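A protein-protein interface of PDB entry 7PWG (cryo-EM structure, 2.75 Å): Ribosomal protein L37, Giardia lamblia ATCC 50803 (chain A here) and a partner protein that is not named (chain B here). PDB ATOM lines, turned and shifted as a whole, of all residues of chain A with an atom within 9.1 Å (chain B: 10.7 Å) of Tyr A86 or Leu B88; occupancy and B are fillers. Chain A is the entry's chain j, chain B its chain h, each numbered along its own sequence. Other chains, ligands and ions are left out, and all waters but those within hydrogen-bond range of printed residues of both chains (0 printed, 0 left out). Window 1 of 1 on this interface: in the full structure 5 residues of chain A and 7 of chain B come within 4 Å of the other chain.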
ATOM      1  N   HIS A  66     -29.993   9.832  -6.025  1.00  0.00           N
ATOM      2  CA  HIS A  66     -29.624   9.242  -4.744  1.00  0.00           C
ATOM      3  C   HIS A  66     -29.746  10.247  -3.610  1.00  0.00           C
ATOM      4  O   HIS A  66     -30.311   9.942  -2.559  1.00  0.00           O
ATOM      5  CB  HIS A  66     -28.204   8.674  -4.806  1.00  0.00           C
ATOM      6  CG  HIS A  66     -27.719   8.134  -3.499  1.00  0.00           C
ATOM      7  ND1 HIS A  66     -28.066   6.884  -3.038  1.00  0.00           N
ATOM      8  CD2 HIS A  66     -26.945   8.686  -2.540  1.00  0.00           C
ATOM      9  CE1 HIS A  66     -27.515   6.684  -1.856  1.00  0.00           C
ATOM     10  NE2 HIS A  66     -26.832   7.763  -1.531  1.00  0.00           N
ATOM     11  N   VAL A  70     -31.848  10.039   0.222  1.00  0.00           N
ATOM     12  CA  VAL A  70     -31.148  10.053   1.505  1.00  0.00           C
ATOM     13  C   VAL A  70     -31.648  11.194   2.384  1.00  0.00           C
ATOM     14  O   VAL A  70     -31.854  11.014   3.586  1.00  0.00           O
ATOM     15  CB  VAL A  70     -29.622  10.126   1.288  1.00  0.00           C
ATOM     16  CG1 VAL A  70     -28.895  10.307   2.606  1.00  0.00           C
ATOM     17  CG2 VAL A  70     -29.117   8.888   0.627  1.00  0.00           C
ATOM     18  N   TYR A  74     -33.626  10.989   6.070  1.00  0.00           N
ATOM     19  CA  TYR A  74     -33.099  11.649   7.260  1.00  0.00           C
ATOM     20  C   TYR A  74     -34.130  12.584   7.877  1.00  0.00           C
ATOM     21  O   TYR A  74     -34.396  12.523   9.081  1.00  0.00           O
ATOM     22  CB  TYR A  74     -31.833  12.413   6.894  1.00  0.00           C
ATOM     23  CG  TYR A  74     -30.997  12.867   8.059  1.00  0.00           C
ATOM     24  CD1 TYR A  74     -31.239  14.080   8.671  1.00  0.00           C
ATOM     25  CD2 TYR A  74     -29.948  12.095   8.530  1.00  0.00           C
ATOM     26  CE1 TYR A  74     -30.488  14.503   9.722  1.00  0.00           C
ATOM     27  CE2 TYR A  74     -29.186  12.519   9.589  1.00  0.00           C
ATOM     28  CZ  TYR A  74     -29.470  13.729  10.180  1.00  0.00           C
ATOM     29  OH  TYR A  74     -28.726  14.183  11.234  1.00  0.00           O
ATOM     30  N   THR A  78     -36.781   7.060   8.836  1.00  0.00           N
ATOM     31  CA  THR A  78     -36.336   6.296  10.000  1.00  0.00           C
ATOM     32  C   THR A  78     -34.820   6.208  10.119  1.00  0.00           C
ATOM     33  O   THR A  78     -34.317   5.392  10.895  1.00  0.00           O
ATOM     34  CB  THR A  78     -36.905   4.875   9.975  1.00  0.00           C
ATOM     35  OG1 THR A  78     -36.219   4.100   8.986  1.00  0.00           O
ATOM     36  CG2 THR A  78     -38.401   4.892   9.658  1.00  0.00           C
ATOM     37  N   LEU A  79     -34.078   7.030   9.388  1.00  0.00           N
ATOM     38  CA  LEU A  79     -32.638   6.838   9.309  1.00  0.00           C
ATOM     39  C   LEU A  79     -31.937   7.256  10.598  1.00  0.00           C
ATOM     40  O   LEU A  79     -30.962   6.621  11.009  1.00  0.00           O
ATOM     41  CB  LEU A  79     -32.102   7.607   8.111  1.00  0.00           C
ATOM     42  CG  LEU A  79     -30.710   7.293   7.607  1.00  0.00           C
ATOM     43  CD1 LEU A  79     -30.629   5.855   7.186  1.00  0.00           C
ATOM     44  CD2 LEU A  79     -30.411   8.204   6.452  1.00  0.00           C
ATOM     45  N   LYS A  80     -32.413   8.317  11.254  1.00  0.00           N
ATOM     46  CA  LYS A  80     -31.794   8.743  12.507  1.00  0.00           C
ATOM     47  C   LYS A  80     -31.995   7.721  13.618  1.00  0.00           C
ATOM     48  O   LYS A  80     -31.161   7.621  14.520  1.00  0.00           O
ATOM     49  CB  LYS A  80     -32.330  10.115  12.928  1.00  0.00           C
ATOM     50  CG  LYS A  80     -31.835  11.248  12.036  1.00  0.00           C
ATOM     51  CD  LYS A  80     -32.039  12.615  12.652  1.00  0.00           C
ATOM     52  CE  LYS A  80     -30.861  12.993  13.525  1.00  0.00           C
ATOM     53  NZ  LYS A  80     -30.974  14.378  14.036  1.00  0.00           N
ATOM     54  N   ALA A  81     -33.084   6.958  13.581  1.00  0.00           N
ATOM     55  CA  ALA A  81     -33.208   5.826  14.490  1.00  0.00           C
ATOM     56  C   ALA A  81     -32.203   4.726  14.157  1.00  0.00           C
ATOM     57  O   ALA A  81     -31.653   4.093  15.062  1.00  0.00           O
ATOM     58  CB  ALA A  81     -34.626   5.271  14.452  1.00  0.00           C
ATOM     59  N   ASN A  82     -31.973   4.460  12.869  1.00  0.00           N
ATOM     60  CA  ASN A  82     -31.100   3.350  12.493  1.00  0.00           C
ATOM     61  C   ASN A  82     -29.669   3.572  12.946  1.00  0.00           C
ATOM     62  O   ASN A  82     -28.925   2.605  13.129  1.00  0.00           O
ATOM     63  CB  ASN A  82     -31.118   3.126  10.980  1.00  0.00           C
ATOM     64  CG  ASN A  82     -32.315   2.322  10.514  1.00  0.00           C
ATOM     65  OD1 ASN A  82     -33.215   2.031  11.286  1.00  0.00           O
ATOM     66  ND2 ASN A  82     -32.328   1.967   9.241  1.00  0.00           N
ATOM     67  N   ALA A  83     -29.253   4.824  13.118  1.00  0.00           N
ATOM     68  CA  ALA A  83     -27.905   5.066  13.614  1.00  0.00           C
ATOM     69  C   ALA A  83     -27.792   4.741  15.096  1.00  0.00           C
ATOM     70  O   ALA A  83     -26.761   4.228  15.542  1.00  0.00           O
ATOM     71  CB  ALA A  83     -27.483   6.506  13.336  1.00  0.00           C
ATOM     72  N   ARG A  84     -28.844   5.008  15.872  1.00  0.00           N
ATOM     73  CA  ARG A  84     -28.792   4.734  17.305  1.00  0.00           C
ATOM     74  C   ARG A  84     -28.640   3.243  17.591  1.00  0.00           C
ATOM     75  O   ARG A  84     -27.861   2.851  18.465  1.00  0.00           O
ATOM     76  CB  ARG A  84     -30.033   5.302  17.991  1.00  0.00           C
ATOM     77  N   LYS A  85     -29.368   2.391  16.868  1.00  0.00           N
ATOM     78  CA  LYS A  85     -29.168   0.953  17.034  1.00  0.00           C
ATOM     79  C   LYS A  85     -27.745   0.548  16.668  1.00  0.00           C
ATOM     80  O   LYS A  85     -27.117  -0.251  17.370  1.00  0.00           O
ATOM     81  CB  LYS A  85     -30.174   0.172  16.190  1.00  0.00           C
ATOM     82  N   TYR A  86     -27.217   1.088  15.572  1.00  0.00           N
ATOM     83  CA  TYR A  86     -25.876   0.716  15.134  1.00  0.00           C
ATOM     84  C   TYR A  86     -24.808   1.321  16.034  1.00  0.00           C
ATOM     85  O   TYR A  86     -23.868   0.633  16.443  1.00  0.00           O
ATOM     86  CB  TYR A  86     -25.671   1.147  13.684  1.00  0.00           C
ATOM     87  CG  TYR A  86     -24.336   0.789  13.099  1.00  0.00           C
ATOM     88  CD1 TYR A  86     -24.070  -0.508  12.666  1.00  0.00           C
ATOM     89  CD2 TYR A  86     -23.343   1.747  12.949  1.00  0.00           C
ATOM     90  CE1 TYR A  86     -22.851  -0.839  12.119  1.00  0.00           C
ATOM     91  CE2 TYR A  86     -22.110   1.419  12.402  1.00  0.00           C
ATOM     92  CZ  TYR A  86     -21.876   0.128  11.987  1.00  0.00           C
ATOM     93  OH  TYR A  86     -20.653  -0.200  11.434  1.00  0.00           O
ATOM     94  N   LEU A  87     -24.936   2.602  16.367  1.00  0.00           N
ATOM     95  CA  LEU A  87     -23.908   3.267  17.157  1.00  0.00           C
ATOM     96  C   LEU A  87     -24.068   2.989  18.642  1.00  0.00           C
ATOM     97  O   LEU A  87     -23.924   3.899  19.458  1.00  0.00           O
ATOM     98  CB  LEU A  87     -23.930   4.778  16.921  1.00  0.00           C
ATOM     99  CG  LEU A  87     -23.175   5.273  15.685  1.00  0.00           C
ATOM    100  CD1 LEU A  87     -21.795   4.674  15.673  1.00  0.00           C
ATOM    101  CD2 LEU A  87     -23.922   4.955  14.399  1.00  0.00           C
ATOM    102  N   ALA A  88     -24.322   1.735  18.994  1.00  0.00           N
ATOM    103  CA  ALA A  88     -24.454   1.306  20.375  1.00  0.00           C
ATOM    104  C   ALA A  88     -23.725  -0.020  20.602  1.00  0.00           C
ATOM    105  O   ALA A  88     -23.932  -1.001  19.879  1.00  0.00           O
ATOM    106  CB  ALA A  88     -25.906   1.174  20.745  1.00  0.00           C
ATOM    107  N   GLU B  78     -19.783 -14.061  10.486  1.00  0.00           N
ATOM    108  CA  GLU B  78     -19.062 -12.847  10.846  1.00  0.00           C
ATOM    109  C   GLU B  78     -19.082 -11.829   9.715  1.00  0.00           C
ATOM    110  O   GLU B  78     -19.302 -10.639   9.958  1.00  0.00           O
ATOM    111  CB  GLU B  78     -17.620 -13.165  11.238  1.00  0.00           C
ATOM    112  CG  GLU B  78     -16.769 -11.927  11.525  1.00  0.00           C
ATOM    113  CD  GLU B  78     -17.392 -11.029  12.591  1.00  0.00           C
ATOM    114  OE1 GLU B  78     -17.948 -11.569  13.573  1.00  0.00           O
ATOM    115  OE2 GLU B  78     -17.344  -9.785  12.443  1.00  0.00           O
ATOM    116  N   ILE B  80     -20.813 -10.560   6.220  1.00  0.00           N
ATOM    117  CA  ILE B  80     -22.137 -10.580   5.612  1.00  0.00           C
ATOM    118  C   ILE B  80     -22.006  -9.927   4.244  1.00  0.00           C
ATOM    119  O   ILE B  80     -21.182  -9.017   4.086  1.00  0.00           O
ATOM    120  CB  ILE B  80     -23.145  -9.848   6.516  1.00  0.00           C
ATOM    121  CG1 ILE B  80     -23.289 -10.585   7.838  1.00  0.00           C
ATOM    122  CG2 ILE B  80     -24.492  -9.684   5.877  1.00  0.00           C
ATOM    123  CD1 ILE B  80     -23.621 -12.006   7.671  1.00  0.00           C
ATOM    124  N   LYS B  82     -22.698  -7.292   1.364  1.00  0.00           N
ATOM    125  CA  LYS B  82     -22.955  -5.871   1.553  1.00  0.00           C
ATOM    126  C   LYS B  82     -24.379  -5.463   1.206  1.00  0.00           C
ATOM    127  O   LYS B  82     -24.817  -4.386   1.619  1.00  0.00           O
ATOM    128  CB  LYS B  82     -21.953  -5.063   0.736  1.00  0.00           C
ATOM    129  CG  LYS B  82     -20.531  -5.491   0.998  1.00  0.00           C
ATOM    130  CD  LYS B  82     -19.543  -4.450   0.595  1.00  0.00           C
ATOM    131  CE  LYS B  82     -18.248  -4.666   1.315  1.00  0.00           C
ATOM    132  NZ  LYS B  82     -17.190  -3.795   0.815  1.00  0.00           N
ATOM    133  N   THR B  83     -25.116  -6.285   0.465  1.00  0.00           N
ATOM    134  CA  THR B  83     -26.523  -5.973   0.242  1.00  0.00           C
ATOM    135  C   THR B  83     -27.350  -6.168   1.505  1.00  0.00           C
ATOM    136  O   THR B  83     -28.373  -5.504   1.677  1.00  0.00           O
ATOM    137  CB  THR B  83     -27.090  -6.824  -0.888  1.00  0.00           C
ATOM    138  OG1 THR B  83     -26.019  -7.341  -1.675  1.00  0.00           O
ATOM    139  CG2 THR B  83     -27.950  -5.978  -1.778  1.00  0.00           C
ATOM    140  N   PHE B  84     -26.926  -7.055   2.397  1.00  0.00           N
ATOM    141  CA  PHE B  84     -27.693  -7.389   3.584  1.00  0.00           C
ATOM    142  C   PHE B  84     -27.202  -6.667   4.832  1.00  0.00           C
ATOM    143  O   PHE B  84     -27.637  -6.993   5.934  1.00  0.00           O
ATOM    144  CB  PHE B  84     -27.670  -8.897   3.809  1.00  0.00           C
ATOM    145  CG  PHE B  84     -28.252  -9.682   2.681  1.00  0.00           C
ATOM    146  CD1 PHE B  84     -29.462  -9.321   2.124  1.00  0.00           C
ATOM    147  CD2 PHE B  84     -27.592 -10.787   2.176  1.00  0.00           C
ATOM    148  CE1 PHE B  84     -29.999 -10.042   1.091  1.00  0.00           C
ATOM    149  CE2 PHE B  84     -28.126 -11.510   1.144  1.00  0.00           C
ATOM    150  CZ  PHE B  84     -29.328 -11.135   0.596  1.00  0.00           C
ATOM    151  N   ARG B  85     -26.307  -5.725   4.688  1.00  0.00           N
ATOM    152  CA  ARG B  85     -25.816  -4.935   5.801  1.00  0.00           C
ATOM    153  C   ARG B  85     -26.766  -3.780   6.088  1.00  0.00           C
ATOM    154  O   ARG B  85     -27.533  -3.364   5.219  1.00  0.00           O
ATOM    155  CB  ARG B  85     -24.408  -4.421   5.494  1.00  0.00           C
ATOM    156  CG  ARG B  85     -23.363  -5.545   5.440  1.00  0.00           C
ATOM    157  CD  ARG B  85     -21.960  -5.084   5.147  1.00  0.00           C
ATOM    158  NE  ARG B  85     -21.087  -6.234   4.940  1.00  0.00           N
ATOM    159  CZ  ARG B  85     -19.793  -6.179   4.662  1.00  0.00           C
ATOM    160  NH1 ARG B  85     -19.172  -5.021   4.551  1.00  0.00           N
ATOM    161  NH2 ARG B  85     -19.111  -7.298   4.503  1.00  0.00           N
ATOM    162  N   PRO B  86     -26.761  -3.261   7.314  1.00  0.00           N
ATOM    163  CA  PRO B  86     -27.667  -2.164   7.671  1.00  0.00           C
ATOM    164  C   PRO B  86     -27.666  -0.978   6.722  1.00  0.00           C
ATOM    165  O   PRO B  86     -26.695  -0.766   5.991  1.00  0.00           O
ATOM    166  CB  PRO B  86     -27.161  -1.765   9.057  1.00  0.00           C
ATOM    167  CG  PRO B  86     -26.750  -3.021   9.634  1.00  0.00           C
ATOM    168  CD  PRO B  86     -26.154  -3.847   8.516  1.00  0.00           C
ATOM    169  N   ARG B  87     -28.754  -0.201   6.722  1.00  0.00           N
ATOM    170  CA  ARG B  87     -28.887   0.957   5.840  1.00  0.00           C
ATOM    171  C   ARG B  87     -28.415   2.206   6.574  1.00  0.00           C
ATOM    172  O   ARG B  87     -29.129   2.752   7.417  1.00  0.00           O
ATOM    173  CB  ARG B  87     -30.324   1.117   5.350  1.00  0.00           C
ATOM    174  CG  ARG B  87     -30.416   2.028   4.134  1.00  0.00           C
ATOM    175  CD  ARG B  87     -31.726   2.790   4.013  1.00  0.00           C
ATOM    176  NE  ARG B  87     -31.623   3.791   2.956  1.00  0.00           N
ATOM    177  CZ  ARG B  87     -32.650   4.443   2.425  1.00  0.00           C
ATOM    178  NH1 ARG B  87     -33.878   4.206   2.847  1.00  0.00           N
ATOM    179  NH2 ARG B  87     -32.444   5.331   1.465  1.00  0.00           N
ATOM    180  N   LEU B  88     -27.216   2.674   6.233  1.00  0.00           N
ATOM    181  CA  LEU B  88     -26.583   3.821   6.867  1.00  0.00           C
ATOM    182  C   LEU B  88     -25.821   4.610   5.811  1.00  0.00           C
ATOM    183  O   LEU B  88     -25.471   4.080   4.758  1.00  0.00           O
ATOM    184  CB  LEU B  88     -25.616   3.384   7.968  1.00  0.00           C
ATOM    185  CG  LEU B  88     -26.050   2.367   9.017  1.00  0.00           C
ATOM    186  CD1 LEU B  88     -24.841   1.644   9.580  1.00  0.00           C
ATOM    187  CD2 LEU B  88     -26.819   3.060  10.117  1.00  0.00           C
ATOM    188  N   THR B  89     -25.543   5.876   6.103  1.00  0.00           N
ATOM    189  CA  THR B  89     -24.750   6.678   5.181  1.00  0.00           C
ATOM    190  C   THR B  89     -23.279   6.314   5.286  1.00  0.00           C
ATOM    191  O   THR B  89     -22.859   5.574   6.166  1.00  0.00           O
ATOM    192  CB  THR B  89     -24.925   8.179   5.434  1.00  0.00           C
ATOM    193  OG1 THR B  89     -24.486   8.518   6.750  1.00  0.00           O
ATOM    194  CG2 THR B  89     -26.345   8.592   5.250  1.00  0.00           C
ATOM    195  N   HIS B  90     -22.492   6.854   4.362  1.00  0.00           N
ATOM    196  CA  HIS B  90     -21.059   6.605   4.366  1.00  0.00           C
ATOM    197  C   HIS B  90     -20.407   7.161   5.623  1.00  0.00           C
ATOM    198  O   HIS B  90     -19.518   6.531   6.195  1.00  0.00           O
ATOM    199  CB  HIS B  90     -20.436   7.205   3.110  1.00  0.00           C
ATOM    200  CG  HIS B  90     -18.958   6.981   2.995  1.00  0.00           C
ATOM    201  ND1 HIS B  90     -18.421   5.911   2.320  1.00  0.00           N
ATOM    202  CD2 HIS B  90     -17.909   7.698   3.456  1.00  0.00           C
ATOM    203  CE1 HIS B  90     -17.105   5.976   2.374  1.00  0.00           C
ATOM    204  NE2 HIS B  90     -16.768   7.052   3.056  1.00  0.00           N
ATOM    205  N   ALA B  91     -20.841   8.335   6.071  1.00  0.00           N
ATOM    206  CA  ALA B  91     -20.283   8.935   7.278  1.00  0.00           C
ATOM    207  C   ALA B  91     -20.650   8.163   8.540  1.00  0.00           C
ATOM    208  O   ALA B  91     -19.862   8.131   9.485  1.00  0.00           O
ATOM    209  CB  ALA B  91     -20.748  10.378   7.414  1.00  0.00           C
ATOM    210  N   MET B  92     -21.845   7.577   8.596  1.00  0.00           N
ATOM    211  CA  MET B  92     -22.254   6.852   9.793  1.00  0.00           C
ATOM    212  C   MET B  92     -21.468   5.564   9.960  1.00  0.00           C
ATOM    213  O   MET B  92     -21.187   5.148  11.084  1.00  0.00           O
ATOM    214  CB  MET B  92     -23.745   6.531   9.745  1.00  0.00           C
ATOM    215  CG  MET B  92     -24.671   7.708   9.776  1.00  0.00           C
ATOM    216  SD  MET B  92     -26.349   7.124   9.510  1.00  0.00           S
ATOM    217  CE  MET B  92     -27.227   8.642   9.214  1.00  0.00           C
ATOM    218  N   ARG B  93     -21.131   4.899   8.856  1.00  0.00           N
ATOM    219  CA  ARG B  93     -20.373   3.662   8.953  1.00  0.00           C
ATOM    220  C   ARG B  93     -18.991   3.895   9.538  1.00  0.00           C
ATOM    221  O   ARG B  93     -18.407   2.967  10.097  1.00  0.00           O
ATOM    222  CB  ARG B  93     -20.263   2.984   7.581  1.00  0.00           C
ATOM    223  CG  ARG B  93     -21.609   2.749   6.888  1.00  0.00           C
ATOM    224  CD  ARG B  93     -21.571   1.678   5.822  1.00  0.00           C
ATOM    225  NE  ARG B  93     -20.966   2.089   4.563  1.00  0.00           N
ATOM    226  CZ  ARG B  93     -21.640   2.532   3.510  1.00  0.00           C
ATOM    227  NH1 ARG B  93     -22.946   2.636   3.557  1.00  0.00           N
ATOM    228  NH2 ARG B  93     -21.003   2.874   2.409  1.00  0.00           N
ATOM    229  N   CYS B  94     -18.484   5.119   9.465  1.00  0.00           N
ATOM    230  CA  CYS B  94     -17.131   5.450   9.882  1.00  0.00           C
ATOM    231  C   CYS B  94     -17.040   6.111  11.254  1.00  0.00           C
ATOM    232  O   CYS B  94     -15.936   6.453  11.675  1.00  0.00           O
ATOM    233  CB  CYS B  94     -16.484   6.362   8.839  1.00  0.00           C
ATOM    234  SG  CYS B  94     -16.054   5.544   7.290  1.00  0.00           S
ATOM    235  N   GLN B  95     -18.156   6.315  11.951  1.00  0.00           N
ATOM    236  CA  GLN B  95     -18.141   6.991  13.243  1.00  0.00           C
ATOM    237  C   GLN B  95     -17.781   6.038  14.375  1.00  0.00           C
ATOM    238  O   GLN B  95     -18.070   4.842  14.324  1.00  0.00           O
ATOM    239  CB  GLN B  95     -19.504   7.596  13.556  1.00  0.00           C
ATOM    240  CG  GLN B  95     -19.844   8.895  12.880  1.00  0.00           C
ATOM    241  CD  GLN B  95     -21.344   9.178  12.946  1.00  0.00           C
ATOM    242  OE1 GLN B  95     -22.061   8.559  13.728  1.00  0.00           O
ATOM    243  NE2 GLN B  95     -21.820  10.098  12.113  1.00  0.00           N
ATOM    244  N   LEU B  96     -17.170   6.590  15.418  1.00  0.00           N
ATOM    245  CA  LEU B  96     -16.936   5.843  16.645  1.00  0.00           C
ATOM    246  C   LEU B  96     -18.257   5.522  17.337  1.00  0.00           C
ATOM    247  O   LEU B  96     -19.236   6.259  17.230  1.00  0.00           O
ATOM    248  CB  LEU B  96     -16.038   6.630  17.602  1.00  0.00           C
ATOM    249  CG  LEU B  96     -14.518   6.633  17.404  1.00  0.00           C
ATOM    250  CD1 LEU B  96     -13.834   7.253  18.606  1.00  0.00           C
ATOM    251  CD2 LEU B  96     -13.992   5.245  17.161  1.00  0.00           C
ATOM    252  N   THR B  97     -18.278   4.395  18.038  1.00  0.00           N
ATOM    253  CA  THR B  97     -19.444   4.001  18.813  1.00  0.00           C
ATOM    254  C   THR B  97     -19.553   4.879  20.058  1.00  0.00           C
ATOM    255  O   THR B  97     -18.571   5.457  20.519  1.00  0.00           O
ATOM    256  CB  THR B  97     -19.339   2.515  19.182  1.00  0.00           C
ATOM    257  OG1 THR B  97     -19.455   1.726  18.000  1.00  0.00           O
ATOM    258  CG2 THR B  97     -20.420   2.083  20.132  1.00  0.00           C
ATOM    259  N   GLU B  98     -20.771   5.013  20.587  1.00  0.00           N
ATOM    260  CA  GLU B  98     -20.954   5.802  21.801  1.00  0.00           C
ATOM    261  C   GLU B  98     -20.148   5.238  22.967  1.00  0.00           C
ATOM    262  O   GLU B  98     -19.651   5.997  23.804  1.00  0.00           O
ATOM    263  CB  GLU B  98     -22.435   5.887  22.150  1.00  0.00           C
ATOM    264  CG  GLU B  98     -23.185   6.919  21.322  1.00  0.00           C
ATOM    265  CD  GLU B  98     -23.015   8.341  21.845  1.00  0.00           C
ATOM    266  OE1 GLU B  98     -22.321   8.537  22.865  1.00  0.00           O
ATOM    267  OE2 GLU B  98     -23.594   9.264  21.234  1.00  0.00           O
ATOM    268  N   LYS B  99     -20.015   3.911  23.048  1.00  0.00           N
ATOM    269  CA  LYS B  99     -19.152   3.319  24.063  1.00  0.00           C
ATOM    270  C   LYS B  99     -17.697   3.687  23.827  1.00  0.00           C
ATOM    271  O   LYS B  99     -16.952   3.946  24.776  1.00  0.00           O
ATOM    272  CB  LYS B  99     -19.304   1.801  24.089  1.00  0.00           C
ATOM    273  CG  LYS B  99     -20.678   1.325  24.467  1.00  0.00           C
ATOM    274  CD  LYS B  99     -20.649  -0.070  25.050  1.00  0.00           C
ATOM    275  CE  LYS B  99     -22.051  -0.585  25.313  1.00  0.00           C
ATOM    276  NZ  LYS B  99     -22.865  -0.777  24.078  1.00  0.00           N
ATOM    277  N   GLN B 100     -17.270   3.685  22.568  1.00  0.00           N
ATOM    278  CA  GLN B 100     -15.895   4.041  22.253  1.00  0.00           C
ATOM    279  C   GLN B 100     -15.615   5.509  22.543  1.00  0.00           C
ATOM    280  O   GLN B 100     -14.503   5.854  22.943  1.00  0.00           O
ATOM    281  CB  GLN B 100     -15.604   3.694  20.795  1.00  0.00           C
ATOM    282  CG  GLN B 100     -15.509   2.202  20.565  1.00  0.00           C
ATOM    283  CD  GLN B 100     -15.446   1.802  19.108  1.00  0.00           C
ATOM    284  OE1 GLN B 100     -16.002   2.466  18.241  1.00  0.00           O
ATOM    285  NE2 GLN B 100     -14.777   0.699  18.838  1.00  0.00           N
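The guanidinium group (NH1) of Arg B93 sits at hydrogen-bond distance from the backbone carbonyl oxygen (O) of Leu B88. The side-chain amide oxygen (OE1) of Gln B100 lies within hydrogen-bond range of the backbone NH (N) of Thr B97 (3.0 Å).
Among the printed residues, pairs that only touch across the chains: Leu A87 with Leu B96 (3.4 Å), Leu A79 with Arg B87 (3.5 Å), Leu A87 with Glu B98 (3.5 Å), Tyr A86 with Leu B88 (3.7 Å), Ala A88 with Lys B99 (3.7 Å), Asn A82 with Leu B88 (3.7 Å), Asn A82 with Arg B87 (3.8 Å), Ala A88 with Thr B97 (3.9 Å), Leu A87 with Gln B95 (3.97 Å) and Leu A87 with Thr B97 (3.98 Å).
Of chain B, only Leu B88 comes within 4 Å of Tyr A86. Of chain B, only Arg B87 and Leu B88 come within 4 Å of Asn A82. No residue of chain B comes within 4 Å of Ala A83. No residue of chain B comes within 4 Å of Arg A84. No residue of chain B comes within 4 Å of Lys A85. Of chain B, only Gln B95 (3.97 Å), Leu B96 (3.4 Å), Thr B97 (3.98 Å) and Glu B98 (3.5 Å) come within 4 Å of Leu A87. No residue of chain A comes within 4 Å of Thr B89. Of the printed residues of chain A, Leu B96 touches Leu A87 (3.4 Å). Of the printed residues of chain A, Arg B87 touches Leu A79 (3.5 Å) and Asn A82 (3.8 Å). Of the printed residues of chain A, Gln B95 touches Leu A87 (3.97 Å). Of the printed residues of chain A, Lys B99 touches Ala A88. Printed residues of chain B within 4 Å of Leu A79: Arg B87.
Printed residues of chain A that touch a printed residue of chain B: Leu A79, Asn A82, Tyr A86, Leu A87 and Ala A88. Hydrophobic or aromatic side chains of chain A that line the printed part of chain B: Leu A79, Tyr A86 and Leu A87. Of the 21 printed residues of chain B, 7 touch a printed residue of chain A. Hydrophobic or aromatic side chains of chain B that line the printed part of chain A: Leu B88. Among the printed residues, 10 pairs touch across the chains. Among the printed residues, no Asp or Glu carboxylate lies within 4 Å of a Lys or Arg side-chain nitrogen of the other chain.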
